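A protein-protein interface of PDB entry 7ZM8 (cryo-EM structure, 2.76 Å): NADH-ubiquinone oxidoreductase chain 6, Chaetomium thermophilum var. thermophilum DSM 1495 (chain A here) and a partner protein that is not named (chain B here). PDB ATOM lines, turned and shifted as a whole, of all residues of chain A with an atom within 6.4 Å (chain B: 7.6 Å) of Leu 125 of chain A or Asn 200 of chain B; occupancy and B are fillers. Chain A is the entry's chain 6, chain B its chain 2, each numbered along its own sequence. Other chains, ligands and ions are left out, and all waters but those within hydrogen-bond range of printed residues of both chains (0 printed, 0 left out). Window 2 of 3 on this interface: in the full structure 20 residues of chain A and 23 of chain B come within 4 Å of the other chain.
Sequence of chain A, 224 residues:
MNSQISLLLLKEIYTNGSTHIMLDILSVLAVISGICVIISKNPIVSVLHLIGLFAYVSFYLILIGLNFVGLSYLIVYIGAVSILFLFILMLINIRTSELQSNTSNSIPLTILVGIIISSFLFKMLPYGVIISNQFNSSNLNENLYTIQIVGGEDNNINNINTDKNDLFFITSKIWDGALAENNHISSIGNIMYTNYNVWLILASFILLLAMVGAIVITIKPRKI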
ATOM      1  N   PHE A 120      18.740   6.776  -4.568  1.00  0.00           N
ATOM      2  CA  PHE A 120      17.331   6.847  -4.933  1.00  0.00           C
ATOM      3  C   PHE A 120      16.672   8.124  -4.427  1.00  0.00           C
ATOM      4  O   PHE A 120      16.031   8.842  -5.200  1.00  0.00           O
ATOM      5  CB  PHE A 120      16.576   5.628  -4.397  1.00  0.00           C
ATOM      6  CG  PHE A 120      16.769   4.392  -5.216  1.00  0.00           C
ATOM      7  CD1 PHE A 120      17.328   4.463  -6.478  1.00  0.00           C
ATOM      8  CD2 PHE A 120      16.388   3.158  -4.725  1.00  0.00           C
ATOM      9  CE1 PHE A 120      17.507   3.324  -7.233  1.00  0.00           C
ATOM     10  CE2 PHE A 120      16.564   2.017  -5.474  1.00  0.00           C
ATOM     11  CZ  PHE A 120      17.123   2.101  -6.730  1.00  0.00           C
ATOM     12  N   LEU A 121      16.821   8.418  -3.134  1.00  0.00           N
ATOM     13  CA  LEU A 121      16.134   9.563  -2.550  1.00  0.00           C
ATOM     14  C   LEU A 121      16.586  10.878  -3.166  1.00  0.00           C
ATOM     15  O   LEU A 121      15.775  11.795  -3.313  1.00  0.00           O
ATOM     16  CB  LEU A 121      16.344   9.587  -1.038  1.00  0.00           C
ATOM     17  CG  LEU A 121      15.286   8.875  -0.194  1.00  0.00           C
ATOM     18  CD1 LEU A 121      15.804   8.596   1.209  1.00  0.00           C
ATOM     19  CD2 LEU A 121      14.013   9.698  -0.140  1.00  0.00           C
ATOM     20  N   PHE A 122      17.853  10.980  -3.570  1.00  0.00           N
ATOM     21  CA  PHE A 122      18.361  12.281  -4.083  1.00  0.00           C
ATOM     22  C   PHE A 122      17.534  12.735  -5.285  1.00  0.00           C
ATOM     23  O   PHE A 122      17.165  13.922  -5.336  1.00  0.00           O
ATOM     24  CB  PHE A 122      19.838  12.178  -4.458  1.00  0.00           C
ATOM     25  CG  PHE A 122      20.438  13.449  -5.002  1.00  0.00           C
ATOM     26  CD1 PHE A 122      20.790  14.487  -4.154  1.00  0.00           C
ATOM     27  CD2 PHE A 122      20.654  13.609  -6.361  1.00  0.00           C
ATOM     28  CE1 PHE A 122      21.343  15.654  -4.654  1.00  0.00           C
ATOM     29  CE2 PHE A 122      21.205  14.778  -6.860  1.00  0.00           C
ATOM     30  CZ  PHE A 122      21.549  15.799  -6.005  1.00  0.00           C
ATOM     31  N   LYS A 123      17.247  11.827  -6.215  1.00  0.00           N
ATOM     32  CA  LYS A 123      16.531  12.211  -7.461  1.00  0.00           C
ATOM     33  C   LYS A 123      15.148  12.738  -7.091  1.00  0.00           C
ATOM     34  O   LYS A 123      14.657  13.643  -7.784  1.00  0.00           O
ATOM     35  CB  LYS A 123      16.439  11.006  -8.400  1.00  0.00           C
ATOM     36  CG  LYS A 123      17.754  10.285  -8.658  1.00  0.00           C
ATOM     37  CD  LYS A 123      18.797  11.158  -9.320  1.00  0.00           C
ATOM     38  CE  LYS A 123      20.130  10.460  -9.493  1.00  0.00           C
ATOM     39  NZ  LYS A 123      20.715  10.066  -8.189  1.00  0.00           N
ATOM     40  N   MET A 124      14.547  12.178  -6.049  1.00  0.00           N
ATOM     41  CA  MET A 124      13.173  12.547  -5.619  1.00  0.00           C
ATOM     42  C   MET A 124      13.036  13.992  -5.148  1.00  0.00           C
ATOM     43  O   MET A 124      11.909  14.458  -5.115  1.00  0.00           O
ATOM     44  CB  MET A 124      12.766  11.601  -4.490  1.00  0.00           C
ATOM     45  CG  MET A 124      12.636  10.211  -5.029  1.00  0.00           C
ATOM     46  SD  MET A 124      11.671  10.237  -6.567  1.00  0.00           S
ATOM     47  CE  MET A 124      12.620   9.096  -7.570  1.00  0.00           C
ATOM     48  N   LEU A 125      14.054  14.631  -4.704  1.00  0.00           N
ATOM     49  CA  LEU A 125      13.914  15.971  -4.102  1.00  0.00           C
ATOM     50  C   LEU A 125      13.567  17.008  -5.177  1.00  0.00           C
ATOM     51  O   LEU A 125      13.916  16.762  -6.341  1.00  0.00           O
ATOM     52  CB  LEU A 125      15.228  16.317  -3.395  1.00  0.00           C
ATOM     53  CG  LEU A 125      15.721  15.281  -2.389  1.00  0.00           C
ATOM     54  CD1 LEU A 125      17.135  15.600  -1.929  1.00  0.00           C
ATOM     55  CD2 LEU A 125      14.780  15.190  -1.198  1.00  0.00           C
ATOM     56  N   PRO A 126      12.973  18.148  -4.888  1.00  0.00           N
ATOM     57  CA  PRO A 126      12.723  19.197  -5.891  1.00  0.00           C
ATOM     58  C   PRO A 126      13.958  20.030  -6.282  1.00  0.00           C
ATOM     59  O   PRO A 126      14.982  19.902  -5.634  1.00  0.00           O
ATOM     60  CB  PRO A 126      11.725  20.074  -5.147  1.00  0.00           C
ATOM     61  CG  PRO A 126      12.151  20.002  -3.725  1.00  0.00           C
ATOM     62  CD  PRO A 126      12.405  18.528  -3.574  1.00  0.00           C
ATOM     63  N   TYR A 127      13.870  20.823  -7.352  1.00  0.00           N
ATOM     64  CA  TYR A 127      15.063  21.574  -7.823  1.00  0.00           C
ATOM     65  C   TYR A 127      15.567  22.571  -6.775  1.00  0.00           C
ATOM     66  O   TYR A 127      16.791  22.681  -6.609  1.00  0.00           O
ATOM     67  CB  TYR A 127      14.797  22.278  -9.149  1.00  0.00           C
ATOM     68  CG  TYR A 127      16.038  22.397  -9.993  1.00  0.00           C
ATOM     69  CD1 TYR A 127      16.746  21.265 -10.353  1.00  0.00           C
ATOM     70  CD2 TYR A 127      16.522  23.628 -10.406  1.00  0.00           C
ATOM     71  CE1 TYR A 127      17.897  21.345 -11.115  1.00  0.00           C
ATOM     72  CE2 TYR A 127      17.671  23.725 -11.172  1.00  0.00           C
ATOM     73  CZ  TYR A 127      18.361  22.579 -11.526  1.00  0.00           C
ATOM     74  OH  TYR A 127      19.499  22.648 -12.275  1.00  0.00           O
ATOM     75  N   VAL A 129      15.669  22.464  -3.589  1.00  0.00           N
ATOM     76  CA  VAL A 129      16.440  21.948  -2.420  1.00  0.00           C
ATOM     77  C   VAL A 129      17.877  21.673  -2.860  1.00  0.00           C
ATOM     78  O   VAL A 129      18.799  21.867  -2.042  1.00  0.00           O
ATOM     79  CB  VAL A 129      15.764  20.692  -1.835  1.00  0.00           C
ATOM     80  CG1 VAL A 129      16.683  19.895  -0.921  1.00  0.00           C
ATOM     81  CG2 VAL A 129      14.478  21.049  -1.109  1.00  0.00           C
ATOM     82  N   ILE A 130      18.056  21.291  -4.130  1.00  0.00           N
ATOM     83  CA  ILE A 130      19.375  20.955  -4.647  1.00  0.00           C
ATOM     84  C   ILE A 130      19.915  22.047  -5.574  1.00  0.00           C
ATOM     85  O   ILE A 130      20.823  21.791  -6.364  1.00  0.00           O
ATOM     86  CB  ILE A 130      19.373  19.588  -5.346  1.00  0.00           C
ATOM     87  CG1 ILE A 130      18.438  19.609  -6.557  1.00  0.00           C
ATOM     88  CG2 ILE A 130      18.962  18.496  -4.374  1.00  0.00           C
ATOM     89  CD1 ILE A 130      18.511  18.358  -7.403  1.00  0.00           C
ATOM     90  N   LEU B 192       7.924  10.227   5.803  1.00  0.00           N
ATOM     91  CA  LEU B 192       8.772  10.487   4.646  1.00  0.00           C
ATOM     92  C   LEU B 192       7.957  10.505   3.364  1.00  0.00           C
ATOM     93  O   LEU B 192       8.187  11.340   2.485  1.00  0.00           O
ATOM     94  CB  LEU B 192       9.876   9.437   4.547  1.00  0.00           C
ATOM     95  CG  LEU B 192      10.823   9.613   3.358  1.00  0.00           C
ATOM     96  CD1 LEU B 192      11.608  10.900   3.470  1.00  0.00           C
ATOM     97  CD2 LEU B 192      11.755   8.436   3.216  1.00  0.00           C
ATOM     98  N   THR B 194       4.712  11.243   2.816  1.00  0.00           N
ATOM     99  CA  THR B 194       3.895  12.441   2.660  1.00  0.00           C
ATOM    100  C   THR B 194       4.759  13.677   2.464  1.00  0.00           C
ATOM    101  O   THR B 194       4.402  14.571   1.691  1.00  0.00           O
ATOM    102  CB  THR B 194       2.975  12.619   3.866  1.00  0.00           C
ATOM    103  OG1 THR B 194       3.765  12.774   5.049  1.00  0.00           O
ATOM    104  CG2 THR B 194       2.075  11.428   4.026  1.00  0.00           C
ATOM    105  N   SER B 195       5.895  13.746   3.154  1.00  0.00           N
ATOM    106  CA  SER B 195       6.803  14.873   2.978  1.00  0.00           C
ATOM    107  C   SER B 195       7.298  14.965   1.543  1.00  0.00           C
ATOM    108  O   SER B 195       7.340  16.054   0.963  1.00  0.00           O
ATOM    109  CB  SER B 195       7.983  14.747   3.936  1.00  0.00           C
ATOM    110  OG  SER B 195       9.005  13.949   3.369  1.00  0.00           O
ATOM    111  N   LEU B 196       7.679  13.835   0.953  1.00  0.00           N
ATOM    112  CA  LEU B 196       8.150  13.839  -0.424  1.00  0.00           C
ATOM    113  C   LEU B 196       7.039  14.140  -1.413  1.00  0.00           C
ATOM    114  O   LEU B 196       7.326  14.543  -2.543  1.00  0.00           O
ATOM    115  CB  LEU B 196       8.792  12.498  -0.762  1.00  0.00           C
ATOM    116  CG  LEU B 196      10.237  12.338  -0.314  1.00  0.00           C
ATOM    117  CD1 LEU B 196      10.635  10.902  -0.465  1.00  0.00           C
ATOM    118  CD2 LEU B 196      11.133  13.230  -1.123  1.00  0.00           C
ATOM    119  N   LEU B 197       5.784  13.942  -1.021  1.00  0.00           N
ATOM    120  CA  LEU B 197       4.679  14.330  -1.885  1.00  0.00           C
ATOM    121  C   LEU B 197       4.522  15.840  -1.926  1.00  0.00           C
ATOM    122  O   LEU B 197       4.365  16.422  -3.003  1.00  0.00           O
ATOM    123  CB  LEU B 197       3.390  13.671  -1.407  1.00  0.00           C
ATOM    124  CG  LEU B 197       3.159  12.254  -1.913  1.00  0.00           C
ATOM    125  CD1 LEU B 197       2.213  11.510  -0.997  1.00  0.00           C
ATOM    126  CD2 LEU B 197       2.639  12.281  -3.325  1.00  0.00           C
ATOM    127  N   TYR B 198       4.585  16.490  -0.766  1.00  0.00           N
ATOM    128  CA  TYR B 198       4.331  17.923  -0.691  1.00  0.00           C
ATOM    129  C   TYR B 198       5.455  18.729  -1.336  1.00  0.00           C
ATOM    130  O   TYR B 198       5.197  19.733  -2.002  1.00  0.00           O
ATOM    131  CB  TYR B 198       4.119  18.321   0.774  1.00  0.00           C
ATOM    132  CG  TYR B 198       4.149  19.801   1.052  1.00  0.00           C
ATOM    133  CD1 TYR B 198       3.059  20.605   0.764  1.00  0.00           C
ATOM    134  CD2 TYR B 198       5.268  20.392   1.616  1.00  0.00           C
ATOM    135  CE1 TYR B 198       3.085  21.949   1.013  1.00  0.00           C
ATOM    136  CE2 TYR B 198       5.306  21.744   1.867  1.00  0.00           C
ATOM    137  CZ  TYR B 198       4.210  22.516   1.567  1.00  0.00           C
ATOM    138  OH  TYR B 198       4.244  23.864   1.821  1.00  0.00           O
ATOM    139  N   VAL B 199       6.690  18.250  -1.247  1.00  0.00           N
ATOM    140  CA  VAL B 199       7.874  18.987  -1.767  1.00  0.00           C
ATOM    141  C   VAL B 199       7.913  18.968  -3.295  1.00  0.00           C
ATOM    142  O   VAL B 199       8.559  19.836  -3.871  1.00  0.00           O
ATOM    143  CB  VAL B 199       9.188  18.469  -1.149  1.00  0.00           C
ATOM    144  CG1 VAL B 199       9.177  18.577   0.366  1.00  0.00           C
ATOM    145  CG2 VAL B 199       9.536  17.059  -1.588  1.00  0.00           C
ATOM    146  N   ASN B 200       7.237  18.012  -3.920  1.00  0.00           N
ATOM    147  CA  ASN B 200       7.291  17.876  -5.392  1.00  0.00           C
ATOM    148  C   ASN B 200       6.006  18.368  -6.023  1.00  0.00           C
ATOM    149  O   ASN B 200       5.989  18.514  -7.237  1.00  0.00           O
ATOM    150  CB  ASN B 200       7.631  16.446  -5.789  1.00  0.00           C
ATOM    151  CG  ASN B 200       9.083  16.088  -5.557  1.00  0.00           C
ATOM    152  OD1 ASN B 200       9.975  16.678  -6.153  1.00  0.00           O
ATOM    153  ND2 ASN B 200       9.329  15.112  -4.702  1.00  0.00           N
ATOM    154  N   SER B 201       4.992  18.649  -5.222  1.00  0.00           N
ATOM    155  CA  SER B 201       3.661  19.023  -5.742  1.00  0.00           C
ATOM    156  C   SER B 201       3.192  20.364  -5.193  1.00  0.00           C
ATOM    157  O   SER B 201       2.296  20.938  -5.794  1.00  0.00           O
ATOM    158  CB  SER B 201       2.712  17.966  -5.347  1.00  0.00           C
ATOM    159  OG  SER B 201       2.514  17.973  -3.949  1.00  0.00           O
ATOM    160  N   GLY B 202       3.709  20.817  -4.064  1.00  0.00           N
ATOM    161  CA  GLY B 202       3.230  22.046  -3.406  1.00  0.00           C
ATOM    162  C   GLY B 202       1.883  21.897  -2.741  1.00  0.00           C
ATOM    163  O   GLY B 202       1.377  22.896  -2.259  1.00  0.00           O
ATOM    164  N   THR B 203       1.336  20.692  -2.681  1.00  0.00           N
ATOM    165  CA  THR B 203      -0.038  20.501  -2.181  1.00  0.00           C
ATOM    166  C   THR B 203      -0.065  19.468  -1.072  1.00  0.00           C
ATOM    167  O   THR B 203       0.825  18.623  -1.051  1.00  0.00           O
ATOM    168  CB  THR B 203      -0.987  20.048  -3.305  1.00  0.00           C
ATOM    169  OG1 THR B 203      -2.321  20.071  -2.796  1.00  0.00           O
ATOM    170  CG2 THR B 203      -0.684  18.689  -3.891  1.00  0.00           C
ATOM    171  N   LEU B 209      -3.414  16.136  -5.816  1.00  0.00           N
ATOM    172  CA  LEU B 209      -2.470  15.069  -6.216  1.00  0.00           C
ATOM    173  C   LEU B 209      -3.151  14.131  -7.205  1.00  0.00           C
ATOM    174  O   LEU B 209      -2.458  13.648  -8.106  1.00  0.00           O
ATOM    175  CB  LEU B 209      -2.091  14.312  -4.946  1.00  0.00           C
ATOM    176  CG  LEU B 209      -1.021  14.971  -4.079  1.00  0.00           C
ATOM    177  CD1 LEU B 209      -0.933  14.295  -2.721  1.00  0.00           C
ATOM    178  CD2 LEU B 209       0.330  14.945  -4.777  1.00  0.00           C
ATOM    179  N   LEU B 212      -3.264  16.046 -10.484  1.00  0.00           N
ATOM    180  CA  LEU B 212      -1.896  16.111 -11.061  1.00  0.00           C
ATOM    181  C   LEU B 212      -1.591  14.759 -11.702  1.00  0.00           C
ATOM    182  O   LEU B 212      -1.050  14.749 -12.813  1.00  0.00           O
ATOM    183  CB  LEU B 212      -0.886  16.460  -9.962  1.00  0.00           C
ATOM    184  CG  LEU B 212      -0.895  17.910  -9.482  1.00  0.00           C
ATOM    185  CD1 LEU B 212      -0.007  18.083  -8.260  1.00  0.00           C
ATOM    186  CD2 LEU B 212      -0.465  18.855 -10.591  1.00  0.00           C
ATOM    187  N   TYR B 235       9.281  18.249 -16.236  1.00  0.00           N
ATOM    188  CA  TYR B 235       8.725  17.823 -14.930  1.00  0.00           C
ATOM    189  C   TYR B 235       7.921  16.543 -15.124  1.00  0.00           C
ATOM    190  O   TYR B 235       6.697  16.592 -15.191  1.00  0.00           O
ATOM    191  CB  TYR B 235       7.874  18.933 -14.320  1.00  0.00           C
ATOM    192  CG  TYR B 235       8.622  20.199 -14.014  1.00  0.00           C
ATOM    193  CD1 TYR B 235       9.326  20.335 -12.832  1.00  0.00           C
ATOM    194  CD2 TYR B 235       8.623  21.257 -14.907  1.00  0.00           C
ATOM    195  CE1 TYR B 235      10.021  21.495 -12.544  1.00  0.00           C
ATOM    196  CE2 TYR B 235       9.319  22.418 -14.637  1.00  0.00           C
ATOM    197  CZ  TYR B 235      10.012  22.538 -13.449  1.00  0.00           C
ATOM    198  OH  TYR B 235      10.689  23.680 -13.164  1.00  0.00           O
ATOM    199  N   PRO B 237       6.259  13.273 -13.648  1.00  0.00           N
ATOM    200  CA  PRO B 237       5.830  12.986 -12.257  1.00  0.00           C
ATOM    201  C   PRO B 237       6.232  11.643 -11.626  1.00  0.00           C
ATOM    202  O   PRO B 237       5.382  10.994 -11.060  1.00  0.00           O
ATOM    203  CB  PRO B 237       4.304  13.083 -12.363  1.00  0.00           C
ATOM    204  CG  PRO B 237       4.016  12.523 -13.721  1.00  0.00           C
ATOM    205  CD  PRO B 237       5.133  13.061 -14.585  1.00  0.00           C
ATOM    206  N   TYR B 238       7.516  11.293 -11.680  1.00  0.00           N
ATOM    207  CA  TYR B 238       8.006  10.004 -11.121  1.00  0.00           C
ATOM    208  C   TYR B 238       7.823   9.987  -9.603  1.00  0.00           C
ATOM    209  O   TYR B 238       7.721   8.888  -9.031  1.00  0.00           O
ATOM    210  CB  TYR B 238       9.453   9.749 -11.551  1.00  0.00           C
ATOM    211  CG  TYR B 238       9.610   9.409 -13.011  1.00  0.00           C
ATOM    212  CD1 TYR B 238       9.079   8.240 -13.531  1.00  0.00           C
ATOM    213  CD2 TYR B 238      10.288  10.253 -13.875  1.00  0.00           C
ATOM    214  CE1 TYR B 238       9.215   7.918 -14.871  1.00  0.00           C
ATOM    215  CE2 TYR B 238      10.435   9.943 -15.217  1.00  0.00           C
ATOM    216  CZ  TYR B 238       9.896   8.773 -15.718  1.00  0.00           C
ATOM    217  OH  TYR B 238      10.037   8.464 -17.041  1.00  0.00           O
ATOM    218  N   TYR B 239       7.705  11.163  -8.995  1.00  0.00           N
ATOM    219  CA  TYR B 239       7.630  11.267  -7.518  1.00  0.00           C
ATOM    220  C   TYR B 239       6.379  10.607  -6.956  1.00  0.00           C
ATOM    221  O   TYR B 239       6.486  10.076  -5.860  1.00  0.00           O
ATOM    222  CB  TYR B 239       7.681  12.732  -7.077  1.00  0.00           C
ATOM    223  CG  TYR B 239       6.439  13.544  -7.339  1.00  0.00           C
ATOM    224  CD1 TYR B 239       6.218  14.142  -8.566  1.00  0.00           C
ATOM    225  CD2 TYR B 239       5.490  13.735  -6.347  1.00  0.00           C
ATOM    226  CE1 TYR B 239       5.081  14.892  -8.809  1.00  0.00           C
ATOM    227  CE2 TYR B 239       4.345  14.479  -6.573  1.00  0.00           C
ATOM    228  CZ  TYR B 239       4.142  15.063  -7.809  1.00  0.00           C
ATOM    229  OH  TYR B 239       3.020  15.799  -8.039  1.00  0.00           O
ATOM    230  N   LEU B 240       5.241  10.662  -7.652  1.00  0.00           N
ATOM    231  CA  LEU B 240       3.999  10.141  -7.030  1.00  0.00           C
ATOM    232  C   LEU B 240       4.122   8.637  -6.772  1.00  0.00           C
ATOM    233  O   LEU B 240       3.785   8.209  -5.667  1.00  0.00           O
ATOM    234  CB  LEU B 240       2.807  10.471  -7.919  1.00  0.00           C
ATOM    235  CG  LEU B 240       1.446  10.059  -7.359  1.00  0.00           C
ATOM    236  CD1 LEU B 240       0.666  11.272  -6.876  1.00  0.00           C
ATOM    237  CD2 LEU B 240       0.645   9.284  -8.390  1.00  0.00           C
ATOM    238  N   PHE B 242       6.913   6.905  -6.558  1.00  0.00           N
ATOM    239  CA  PHE B 242       8.010   6.682  -5.580  1.00  0.00           C
ATOM    240  C   PHE B 242       7.535   7.062  -4.170  1.00  0.00           C
ATOM    241  O   PHE B 242       7.798   6.293  -3.230  1.00  0.00           O
ATOM    242  CB  PHE B 242       9.270   7.447  -5.990  1.00  0.00           C
ATOM    243  CG  PHE B 242      10.498   7.153  -5.165  1.00  0.00           C
ATOM    244  CD1 PHE B 242      10.667   7.707  -3.906  1.00  0.00           C
ATOM    245  CD2 PHE B 242      11.501   6.338  -5.659  1.00  0.00           C
ATOM    246  CE1 PHE B 242      11.804   7.442  -3.158  1.00  0.00           C
ATOM    247  CE2 PHE B 242      12.641   6.081  -4.913  1.00  0.00           C
ATOM    248  CZ  PHE B 242      12.789   6.630  -3.662  1.00  0.00           C
ATOM    249  N   SER B 243       6.885   8.221  -4.026  1.00  0.00           N
ATOM    250  CA  SER B 243       6.427   8.643  -2.707  1.00  0.00           C
ATOM    251  C   SER B 243       5.408   7.670  -2.137  1.00  0.00           C
ATOM    252  O   SER B 243       5.476   7.309  -0.959  1.00  0.00           O
ATOM    253  CB  SER B 243       5.839  10.047  -2.776  1.00  0.00           C
ATOM    254  OG  SER B 243       6.839  11.000  -3.061  1.00  0.00           O
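O of Met 124 of chain A lies within hydrogen-bond range of ND2 of Asn 200 of chain B (2.7 Å).
Printed residues of chain B within 4 Å of Leu 121 of chain A: Leu 196.
Of the printed residues of chain B, Met 124 of chain A touches Asn 200 (2.7 Å) and Phe 242 (3.4 Å).
Ile 130 of chain A touches none of the printed residues of chain B.
Printed residues of chain A within 4 Å of Val 199 of chain B: Pro 126.
Asn 200 of chain B touches just these residues of chain A: Met 124 (2.7 Å), Leu 125 (3.7 Å) and Pro 126 (3.6 Å).
Printed residues of chain A within 4 Å of Phe 242 of chain B: Phe 120 and Met 124.
The nearest residue of chain B that does not touch Leu 125 of chain A is Leu 196 of chain B (4.1 Å).
The nearest printed residue of chain A that does not touch Asn 200 of chain B is Tyr 127 of chain A (5.8 Å).
Of the 10 printed residues of chain A, 5 touch a printed residue of chain B.
Hydrophobic or aromatic side chains of chain A that line the printed part of chain B: Phe 120, Leu 121, Met 124 and Pro 126.
Among the printed residues, 7 pairs touch across the chains.
Among the printed residues, no Asp or Glu carboxylate lies within 4 Å of a Lys or Arg side-chain nitrogen of the other chain.
Among the printed residues, merely in contact across the chains: Met 124 of chain A with Phe 242 of chain B, Pro 126 of chain A with Val 199 of chain B, Pro 126 of chain A with Asn 200 of chain B, Leu 121 of chain A with Leu 196 of chain B, Leu 125 of chain A with Asn 200 of chain B and Phe 120 of chain A with Phe 242 of chain B.
The backbone carbonyl oxygen (O) of Leu 196 of chain B is in hydrogen-bond range of the side-chain amide nitrogen (ND2) of Asn 200 of chain B (3.0 Å).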
